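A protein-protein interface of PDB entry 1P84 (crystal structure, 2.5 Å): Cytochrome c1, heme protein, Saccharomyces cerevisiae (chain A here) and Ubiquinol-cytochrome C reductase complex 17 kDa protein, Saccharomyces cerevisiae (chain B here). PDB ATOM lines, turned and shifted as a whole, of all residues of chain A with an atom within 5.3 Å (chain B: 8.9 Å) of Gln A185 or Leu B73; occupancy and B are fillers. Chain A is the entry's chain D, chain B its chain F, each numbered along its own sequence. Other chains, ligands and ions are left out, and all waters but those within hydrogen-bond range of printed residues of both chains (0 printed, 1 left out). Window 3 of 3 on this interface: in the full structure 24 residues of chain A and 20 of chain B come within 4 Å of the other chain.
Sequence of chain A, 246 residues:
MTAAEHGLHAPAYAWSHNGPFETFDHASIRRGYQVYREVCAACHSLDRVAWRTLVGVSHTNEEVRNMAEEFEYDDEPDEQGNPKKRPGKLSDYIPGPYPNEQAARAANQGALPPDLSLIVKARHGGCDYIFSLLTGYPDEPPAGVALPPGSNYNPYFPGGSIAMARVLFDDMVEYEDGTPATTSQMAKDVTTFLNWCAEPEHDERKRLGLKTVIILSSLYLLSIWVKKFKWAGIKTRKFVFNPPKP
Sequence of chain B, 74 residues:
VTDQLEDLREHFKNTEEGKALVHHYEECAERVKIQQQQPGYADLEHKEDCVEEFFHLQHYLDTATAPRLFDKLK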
ATOM      1  N   ARG A  31     -16.520 -10.021 -13.365  1.00  0.00           N
ATOM      2  CA  ARG A  31     -15.312  -9.225 -13.166  1.00  0.00           C
ATOM      3  C   ARG A  31     -15.415  -8.427 -11.870  1.00  0.00           C
ATOM      4  O   ARG A  31     -14.483  -8.419 -11.059  1.00  0.00           O
ATOM      5  CB  ARG A  31     -15.112  -8.255 -14.332  1.00  0.00           C
ATOM      6  CG  ARG A  31     -14.310  -8.798 -15.500  1.00  0.00           C
ATOM      7  CD  ARG A  31     -14.205  -7.766 -16.607  1.00  0.00           C
ATOM      8  NE  ARG A  31     -15.027  -8.120 -17.756  1.00  0.00           N
ATOM      9  CZ  ARG A  31     -15.870  -7.292 -18.362  1.00  0.00           C
ATOM     10  NH1 ARG A  31     -16.573  -7.710 -19.409  1.00  0.00           N
ATOM     11  NH2 ARG A  31     -16.032  -6.056 -17.910  1.00  0.00           N
ATOM     12  N   PHE A 131     -19.880   4.924  -8.986  1.00  0.00           N
ATOM     13  CA  PHE A 131     -18.852   4.996 -10.004  1.00  0.00           C
ATOM     14  C   PHE A 131     -18.109   6.325  -9.909  1.00  0.00           C
ATOM     15  O   PHE A 131     -16.881   6.360  -9.815  1.00  0.00           O
ATOM     16  CB  PHE A 131     -19.476   4.852 -11.393  1.00  0.00           C
ATOM     17  CG  PHE A 131     -18.479   4.962 -12.513  1.00  0.00           C
ATOM     18  CD1 PHE A 131     -17.829   3.831 -12.999  1.00  0.00           C
ATOM     19  CD2 PHE A 131     -18.173   6.200 -13.069  1.00  0.00           C
ATOM     20  CE1 PHE A 131     -16.888   3.930 -14.018  1.00  0.00           C
ATOM     21  CE2 PHE A 131     -17.234   6.311 -14.090  1.00  0.00           C
ATOM     22  CZ  PHE A 131     -16.591   5.169 -14.566  1.00  0.00           C
ATOM     23  N   TYR A 175      -7.552  -9.251 -14.685  1.00  0.00           N
ATOM     24  CA  TYR A 175      -8.819  -9.821 -15.120  1.00  0.00           C
ATOM     25  C   TYR A 175      -8.627 -11.155 -15.822  1.00  0.00           C
ATOM     26  O   TYR A 175      -7.903 -11.264 -16.813  1.00  0.00           O
ATOM     27  CB  TYR A 175      -9.590  -8.854 -16.022  1.00  0.00           C
ATOM     28  CG  TYR A 175     -10.394  -7.802 -15.283  1.00  0.00           C
ATOM     29  CD1 TYR A 175     -10.631  -6.550 -15.857  1.00  0.00           C
ATOM     30  CD2 TYR A 175     -10.937  -8.063 -14.024  1.00  0.00           C
ATOM     31  CE1 TYR A 175     -11.389  -5.586 -15.201  1.00  0.00           C
ATOM     32  CE2 TYR A 175     -11.698  -7.107 -13.359  1.00  0.00           C
ATOM     33  CZ  TYR A 175     -11.920  -5.871 -13.955  1.00  0.00           C
ATOM     34  OH  TYR A 175     -12.679  -4.917 -13.315  1.00  0.00           O
ATOM     35  N   THR A 179      -9.570  -8.729 -20.171  1.00  0.00           N
ATOM     36  CA  THR A 179      -9.886  -7.296 -20.239  1.00  0.00           C
ATOM     37  C   THR A 179      -8.869  -6.382 -19.530  1.00  0.00           C
ATOM     38  O   THR A 179      -8.343  -6.724 -18.461  1.00  0.00           O
ATOM     39  CB  THR A 179     -11.313  -7.037 -19.686  1.00  0.00           C
ATOM     40  OG1 THR A 179     -12.248  -7.877 -20.379  1.00  0.00           O
ATOM     41  CG2 THR A 179     -11.721  -5.571 -19.871  1.00  0.00           C
ATOM     42  N   PRO A 180      -8.539  -5.232 -20.158  1.00  0.00           N
ATOM     43  CA  PRO A 180      -7.587  -4.253 -19.609  1.00  0.00           C
ATOM     44  C   PRO A 180      -8.155  -3.656 -18.322  1.00  0.00           C
ATOM     45  O   PRO A 180      -9.174  -2.962 -18.350  1.00  0.00           O
ATOM     46  CB  PRO A 180      -7.511  -3.187 -20.711  1.00  0.00           C
ATOM     47  CG  PRO A 180      -7.900  -3.926 -21.963  1.00  0.00           C
ATOM     48  CD  PRO A 180      -9.014  -4.812 -21.491  1.00  0.00           C
ATOM     49  N   ALA A 181      -7.490  -3.913 -17.202  1.00  0.00           N
ATOM     50  CA  ALA A 181      -7.957  -3.415 -15.915  1.00  0.00           C
ATOM     51  C   ALA A 181      -7.640  -1.959 -15.569  1.00  0.00           C
ATOM     52  O   ALA A 181      -6.934  -1.684 -14.594  1.00  0.00           O
ATOM     53  CB  ALA A 181      -7.494  -4.338 -14.802  1.00  0.00           C
ATOM     54  N   THR A 182      -8.181  -1.026 -16.352  1.00  0.00           N
ATOM     55  CA  THR A 182      -7.989   0.405 -16.096  1.00  0.00           C
ATOM     56  C   THR A 182      -8.876   0.786 -14.904  1.00  0.00           C
ATOM     57  O   THR A 182      -9.840   0.073 -14.611  1.00  0.00           O
ATOM     58  CB  THR A 182      -8.387   1.245 -17.319  1.00  0.00           C
ATOM     59  OG1 THR A 182      -9.770   1.032 -17.626  1.00  0.00           O
ATOM     60  CG2 THR A 182      -7.549   0.849 -18.526  1.00  0.00           C
ATOM     61  N   THR A 183      -8.585   1.901 -14.229  1.00  0.00           N
ATOM     62  CA  THR A 183      -9.387   2.285 -13.054  1.00  0.00           C
ATOM     63  C   THR A 183     -10.869   2.471 -13.354  1.00  0.00           C
ATOM     64  O   THR A 183     -11.711   2.108 -12.535  1.00  0.00           O
ATOM     65  CB  THR A 183      -8.868   3.555 -12.311  1.00  0.00           C
ATOM     66  OG1 THR A 183      -9.597   4.710 -12.742  1.00  0.00           O
ATOM     67  CG2 THR A 183      -7.389   3.773 -12.564  1.00  0.00           C
ATOM     68  N   SER A 184     -11.186   3.017 -14.526  1.00  0.00           N
ATOM     69  CA  SER A 184     -12.579   3.230 -14.902  1.00  0.00           C
ATOM     70  C   SER A 184     -13.271   1.910 -15.236  1.00  0.00           C
ATOM     71  O   SER A 184     -14.455   1.731 -14.931  1.00  0.00           O
ATOM     72  CB  SER A 184     -12.705   4.220 -16.071  1.00  0.00           C
ATOM     73  OG  SER A 184     -12.221   3.669 -17.281  1.00  0.00           O
ATOM     74  N   GLN A 185     -12.527   0.980 -15.836  1.00  0.00           N
ATOM     75  CA  GLN A 185     -13.073  -0.330 -16.193  1.00  0.00           C
ATOM     76  C   GLN A 185     -13.432  -1.104 -14.939  1.00  0.00           C
ATOM     77  O   GLN A 185     -14.450  -1.792 -14.905  1.00  0.00           O
ATOM     78  CB  GLN A 185     -12.064  -1.135 -17.011  1.00  0.00           C
ATOM     79  CG  GLN A 185     -12.500  -2.563 -17.323  1.00  0.00           C
ATOM     80  CD  GLN A 185     -13.602  -2.652 -18.355  1.00  0.00           C
ATOM     81  OE1 GLN A 185     -13.580  -1.965 -19.371  1.00  0.00           O
ATOM     82  NE2 GLN A 185     -14.562  -3.528 -18.113  1.00  0.00           N
ATOM     83  N   MET A 186     -12.590  -0.988 -13.914  1.00  0.00           N
ATOM     84  CA  MET A 186     -12.823  -1.680 -12.658  1.00  0.00           C
ATOM     85  C   MET A 186     -13.978  -1.074 -11.886  1.00  0.00           C
ATOM     86  O   MET A 186     -14.784  -1.801 -11.313  1.00  0.00           O
ATOM     87  CB  MET A 186     -11.568  -1.686 -11.792  1.00  0.00           C
ATOM     88  CG  MET A 186     -10.459  -2.552 -12.339  1.00  0.00           C
ATOM     89  SD  MET A 186      -9.034  -2.541 -11.276  1.00  0.00           S
ATOM     90  CE  MET A 186      -8.391  -0.908 -11.614  1.00  0.00           C
ATOM     91  N   ALA A 187     -14.054   0.255 -11.862  1.00  0.00           N
ATOM     92  CA  ALA A 187     -15.135   0.937 -11.163  1.00  0.00           C
ATOM     93  C   ALA A 187     -16.442   0.521 -11.826  1.00  0.00           C
ATOM     94  O   ALA A 187     -17.390   0.119 -11.158  1.00  0.00           O
ATOM     95  CB  ALA A 187     -14.952   2.438 -11.254  1.00  0.00           C
ATOM     96  N   LYS A 188     -16.449   0.545 -13.152  1.00  0.00           N
ATOM     97  CA  LYS A 188     -17.617   0.164 -13.927  1.00  0.00           C
ATOM     98  C   LYS A 188     -18.058  -1.257 -13.587  1.00  0.00           C
ATOM     99  O   LYS A 188     -19.255  -1.554 -13.556  1.00  0.00           O
ATOM    100  CB  LYS A 188     -17.300   0.284 -15.415  1.00  0.00           C
ATOM    101  CG  LYS A 188     -18.473   0.105 -16.356  1.00  0.00           C
ATOM    102  CD  LYS A 188     -18.632  -1.331 -16.787  1.00  0.00           C
ATOM    103  CE  LYS A 188     -19.408  -1.427 -18.089  1.00  0.00           C
ATOM    104  NZ  LYS A 188     -19.602  -2.851 -18.483  1.00  0.00           N
ATOM    105  N   ASP A 189     -17.094  -2.120 -13.286  1.00  0.00           N
ATOM    106  CA  ASP A 189     -17.398  -3.505 -12.953  1.00  0.00           C
ATOM    107  C   ASP A 189     -17.940  -3.732 -11.541  1.00  0.00           C
ATOM    108  O   ASP A 189     -19.017  -4.313 -11.407  1.00  0.00           O
ATOM    109  CB  ASP A 189     -16.194  -4.414 -13.247  1.00  0.00           C
ATOM    110  CG  ASP A 189     -15.934  -4.583 -14.748  1.00  0.00           C
ATOM    111  OD1 ASP A 189     -16.829  -4.255 -15.560  1.00  0.00           O
ATOM    112  OD2 ASP A 189     -14.837  -5.048 -15.125  1.00  0.00           O
ATOM    113  N   THR B   2      -3.797   3.354 -20.992  1.00  0.00           N
ATOM    114  CA  THR B   2      -4.089   4.560 -20.228  1.00  0.00           C
ATOM    115  C   THR B   2      -5.594   4.606 -19.909  1.00  0.00           C
ATOM    116  O   THR B   2      -6.424   4.241 -20.752  1.00  0.00           O
ATOM    117  CB  THR B   2      -3.657   5.818 -21.023  1.00  0.00           C
ATOM    118  OG1 THR B   2      -3.924   6.997 -20.255  1.00  0.00           O
ATOM    119  CG2 THR B   2      -4.393   5.904 -22.361  1.00  0.00           C
ATOM    120  N   ASP B   3      -5.939   5.037 -18.692  1.00  0.00           N
ATOM    121  CA  ASP B   3      -7.340   5.117 -18.260  1.00  0.00           C
ATOM    122  C   ASP B   3      -8.242   5.955 -19.171  1.00  0.00           C
ATOM    123  O   ASP B   3      -8.036   7.160 -19.331  1.00  0.00           O
ATOM    124  CB  ASP B   3      -7.446   5.630 -16.823  1.00  0.00           C
ATOM    125  CG  ASP B   3      -8.889   5.796 -16.376  1.00  0.00           C
ATOM    126  OD1 ASP B   3      -9.630   4.794 -16.402  1.00  0.00           O
ATOM    127  OD2 ASP B   3      -9.290   6.929 -16.025  1.00  0.00           O
ATOM    128  N   GLN B   4      -9.291   5.313 -19.684  1.00  0.00           N
ATOM    129  CA  GLN B   4     -10.251   5.928 -20.600  1.00  0.00           C
ATOM    130  C   GLN B   4     -10.929   7.210 -20.116  1.00  0.00           C
ATOM    131  O   GLN B   4     -11.241   8.086 -20.925  1.00  0.00           O
ATOM    132  CB  GLN B   4     -11.316   4.912 -21.020  1.00  0.00           C
ATOM    133  CG  GLN B   4     -10.779   3.657 -21.696  1.00  0.00           C
ATOM    134  CD  GLN B   4     -10.484   2.525 -20.724  1.00  0.00           C
ATOM    135  OE1 GLN B   4     -10.597   1.351 -21.080  1.00  0.00           O
ATOM    136  NE2 GLN B   4     -10.123   2.868 -19.489  1.00  0.00           N
ATOM    137  N   LEU B   5     -11.182   7.313 -18.813  1.00  0.00           N
ATOM    138  CA  LEU B   5     -11.817   8.506 -18.268  1.00  0.00           C
ATOM    139  C   LEU B   5     -10.823   9.668 -18.240  1.00  0.00           C
ATOM    140  O   LEU B   5     -11.143  10.775 -18.675  1.00  0.00           O
ATOM    141  CB  LEU B   5     -12.370   8.242 -16.864  1.00  0.00           C
ATOM    142  CG  LEU B   5     -13.068   9.419 -16.170  1.00  0.00           C
ATOM    143  CD1 LEU B   5     -14.295   9.849 -16.940  1.00  0.00           C
ATOM    144  CD2 LEU B   5     -13.438   9.031 -14.763  1.00  0.00           C
ATOM    145  N   LEU B   8     -10.356  11.091 -21.690  1.00  0.00           N
ATOM    146  CA  LEU B   8     -11.443  11.984 -22.090  1.00  0.00           C
ATOM    147  C   LEU B   8     -11.479  13.306 -21.321  1.00  0.00           C
ATOM    148  O   LEU B   8     -11.881  14.334 -21.871  1.00  0.00           O
ATOM    149  CB  LEU B   8     -12.792  11.270 -21.988  1.00  0.00           C
ATOM    150  CG  LEU B   8     -13.128  10.363 -23.169  1.00  0.00           C
ATOM    151  CD1 LEU B   8     -14.387   9.578 -22.886  1.00  0.00           C
ATOM    152  CD2 LEU B   8     -13.294  11.200 -24.424  1.00  0.00           C
ATOM    153  N   THR B  65     -17.960  14.037 -20.702  1.00  0.00           N
ATOM    154  CA  THR B  65     -17.449  12.677 -20.604  1.00  0.00           C
ATOM    155  C   THR B  65     -18.453  11.568 -20.293  1.00  0.00           C
ATOM    156  O   THR B  65     -18.247  10.421 -20.689  1.00  0.00           O
ATOM    157  CB  THR B  65     -16.286  12.596 -19.599  1.00  0.00           C
ATOM    158  OG1 THR B  65     -16.774  12.800 -18.269  1.00  0.00           O
ATOM    159  CG2 THR B  65     -15.251  13.655 -19.911  1.00  0.00           C
ATOM    160  N   ARG B  68     -20.052   9.486 -23.243  1.00  0.00           N
ATOM    161  CA  ARG B  68     -19.048   8.873 -24.111  1.00  0.00           C
ATOM    162  C   ARG B  68     -18.151   7.815 -23.475  1.00  0.00           C
ATOM    163  O   ARG B  68     -17.700   6.903 -24.163  1.00  0.00           O
ATOM    164  CB  ARG B  68     -18.170   9.960 -24.752  1.00  0.00           C
ATOM    165  CG  ARG B  68     -18.777  10.619 -25.985  1.00  0.00           C
ATOM    166  CD  ARG B  68     -17.893  11.743 -26.519  1.00  0.00           C
ATOM    167  NE  ARG B  68     -18.101  12.997 -25.797  1.00  0.00           N
ATOM    168  CZ  ARG B  68     -18.615  14.102 -26.339  1.00  0.00           C
ATOM    169  NH1 ARG B  68     -18.770  15.195 -25.596  1.00  0.00           N
ATOM    170  NH2 ARG B  68     -18.972  14.123 -27.621  1.00  0.00           N
ATOM    171  N   LEU B  69     -17.912   7.917 -22.171  1.00  0.00           N
ATOM    172  CA  LEU B  69     -17.030   6.981 -21.474  1.00  0.00           C
ATOM    173  C   LEU B  69     -17.305   5.480 -21.612  1.00  0.00           C
ATOM    174  O   LEU B  69     -16.366   4.679 -21.652  1.00  0.00           O
ATOM    175  CB  LEU B  69     -16.925   7.342 -19.990  1.00  0.00           C
ATOM    176  CG  LEU B  69     -16.027   6.404 -19.173  1.00  0.00           C
ATOM    177  CD1 LEU B  69     -14.604   6.416 -19.712  1.00  0.00           C
ATOM    178  CD2 LEU B  69     -16.054   6.783 -17.711  1.00  0.00           C
ATOM    179  N   PHE B  70     -18.571   5.086 -21.676  1.00  0.00           N
ATOM    180  CA  PHE B  70     -18.880   3.666 -21.771  1.00  0.00           C
ATOM    181  C   PHE B  70     -18.736   3.031 -23.148  1.00  0.00           C
ATOM    182  O   PHE B  70     -18.569   1.815 -23.253  1.00  0.00           O
ATOM    183  CB  PHE B  70     -20.235   3.357 -21.127  1.00  0.00           C
ATOM    184  CG  PHE B  70     -20.191   3.350 -19.621  1.00  0.00           C
ATOM    185  CD1 PHE B  70     -19.229   4.083 -18.938  1.00  0.00           C
ATOM    186  CD2 PHE B  70     -21.087   2.593 -18.888  1.00  0.00           C
ATOM    187  CE1 PHE B  70     -19.157   4.060 -17.550  1.00  0.00           C
ATOM    188  CE2 PHE B  70     -21.019   2.567 -17.496  1.00  0.00           C
ATOM    189  CZ  PHE B  70     -20.052   3.300 -16.828  1.00  0.00           C
ATOM    190  N   ASP B  71     -18.774   3.845 -24.199  1.00  0.00           N
ATOM    191  CA  ASP B  71     -18.602   3.328 -25.553  1.00  0.00           C
ATOM    192  C   ASP B  71     -17.164   2.836 -25.722  1.00  0.00           C
ATOM    193  O   ASP B  71     -16.861   2.075 -26.640  1.00  0.00           O
ATOM    194  CB  ASP B  71     -18.901   4.405 -26.602  1.00  0.00           C
ATOM    195  CG  ASP B  71     -20.370   4.458 -26.987  1.00  0.00           C
ATOM    196  OD1 ASP B  71     -20.876   5.576 -27.230  1.00  0.00           O
ATOM    197  OD2 ASP B  71     -21.018   3.388 -27.067  1.00  0.00           O
ATOM    198  N   LYS B  72     -16.285   3.279 -24.826  1.00  0.00           N
ATOM    199  CA  LYS B  72     -14.883   2.889 -24.855  1.00  0.00           C
ATOM    200  C   LYS B  72     -14.570   1.721 -23.916  1.00  0.00           C
ATOM    201  O   LYS B  72     -13.571   1.030 -24.094  1.00  0.00           O
ATOM    202  CB  LYS B  72     -13.996   4.091 -24.516  1.00  0.00           C
ATOM    203  CG  LYS B  72     -14.085   5.238 -25.521  1.00  0.00           C
ATOM    204  CD  LYS B  72     -13.723   4.779 -26.937  1.00  0.00           C
ATOM    205  CE  LYS B  72     -13.749   5.935 -27.930  1.00  0.00           C
ATOM    206  NZ  LYS B  72     -12.758   6.993 -27.570  1.00  0.00           N
ATOM    207  N   LEU B  73     -15.418   1.510 -22.911  1.00  0.00           N
ATOM    208  CA  LEU B  73     -15.220   0.424 -21.955  1.00  0.00           C
ATOM    209  C   LEU B  73     -15.834  -0.880 -22.445  1.00  0.00           C
ATOM    210  O   LEU B  73     -16.576  -0.900 -23.427  1.00  0.00           O
ATOM    211  CB  LEU B  73     -15.811   0.794 -20.594  1.00  0.00           C
ATOM    212  CG  LEU B  73     -15.154   1.962 -19.858  1.00  0.00           C
ATOM    213  CD1 LEU B  73     -15.819   2.179 -18.508  1.00  0.00           C
ATOM    214  CD2 LEU B  73     -13.685   1.676 -19.667  1.00  0.00           C
ATOM    215  N   LYS B  74     -15.495  -1.974 -21.773  1.00  0.00           N
ATOM    216  CA  LYS B  74     -16.024  -3.283 -22.128  1.00  0.00           C
ATOM    217  C   LYS B  74     -17.135  -3.669 -21.147  1.00  0.00           C
ATOM    218  O   LYS B  74     -16.919  -3.540 -19.923  1.00  0.00           O
ATOM    219  CB  LYS B  74     -14.897  -4.333 -22.133  1.00  0.00           C
ATOM    220  CG  LYS B  74     -15.344  -5.777 -22.406  1.00  0.00           C
ATOM    221  CD  LYS B  74     -16.083  -5.931 -23.746  1.00  0.00           C
ATOM    222  CE  LYS B  74     -16.538  -7.382 -23.991  1.00  0.00           C
ATOM    223  NZ  LYS B  74     -17.504  -7.894 -22.962  1.00  0.00           N
ATOM    224  OXT LYS B  74     -18.219  -4.072 -21.619  1.00  0.00           O
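Hydrophobic or aromatic side chains of chain A within 4 Å of the printed part of chain B: Phe A131. Along chain A the printed residues that touch a printed residue of chain B span positions 31 to 188. Of the 13 printed residues of chain B, 6 touch a printed residue of chain A. Hydrophobic or aromatic side chains of chain B that line the printed part of chain A: Leu B69, Phe B70 and Leu B73. Among the printed residues, 13 pairs touch across the chains. Among the printed residues, no Asp or Glu carboxylate lies within 4 Å of a Lys or Arg side-chain nitrogen of the other chain.
O of Lys B74 is in hydrogen-bond range of NE2 of Gln A185 (3.0 Å). The side-chain hydroxyl (OG) of Ser A184 sits at hydrogen-bond distance from the side-chain carboxylate (OD1) of Asp B3 (3.0 Å). O of Lys B74 lies within salt-bridge range of NZ of Lys A188, 3.1 Å away. NE2 of Gln B4 sits at hydrogen-bond distance from OG1 of Thr A182 (2.6 Å). The chain-end carboxylate (O) of Lys B74 lies within salt-bridge range of the guanidinium group (NH2) of Arg A31 (3.3 Å). The side-chain hydroxyl of Ser A184 is in hydrogen-bond range of the side-chain amide nitrogen of Gln B4, 3.1 Å away.
CD2 of Leu B69 touches CZ of Phe A131, at 3.6 Å. CB of Thr A182 touches OD1 of Asp B3 (3.9 Å). Thr A183 touches Asp B3. OG of Ser A184 touches CD2 of Leu B73, at 3.4 Å. Gln A185 touches Leu B73 (OE1 to CD2, 3.7 Å). CG of Lys A188 touches CZ of Phe B70, at 3.6 Å. CB of Lys A188 touches CD1 of Leu B73, at 3.9 Å.
OD1 of Asp A189 lies within salt-bridge range of NH2 of Arg A31 (3.1 Å). NE2 of Gln A185 sits at hydrogen-bond distance from OD2 of Asp A189 (3.4 Å). The side-chain carboxylate (OD2) of Asp B3 lies close to the backbone NH (N) of Leu B5 (3.4 Å). The guanidinium group of Arg A31 lies close to the side-chain amide nitrogen of Gln A185, at 2.9 Å. OG1 of Thr A182 sits close to N of Gln A185 (3.3 Å).
Gln A185 touches just these residues of chain B: Leu B73 (3.7 Å) and Lys B74 (3.0 Å). Leu B73 touches three residues of chain A. Of the printed residues of chain A, Phe B70 touches Lys A188. Of the printed residues of chain A, Asp B3 touches Thr A182, Thr A183 and Ser A184. Leu B5 touches none of the printed residues of chain A. Thr A179 touches none of the printed residues of chain B. The nearest residue of chain A that does not touch Leu B73 is Thr A182 (4.5 Å).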
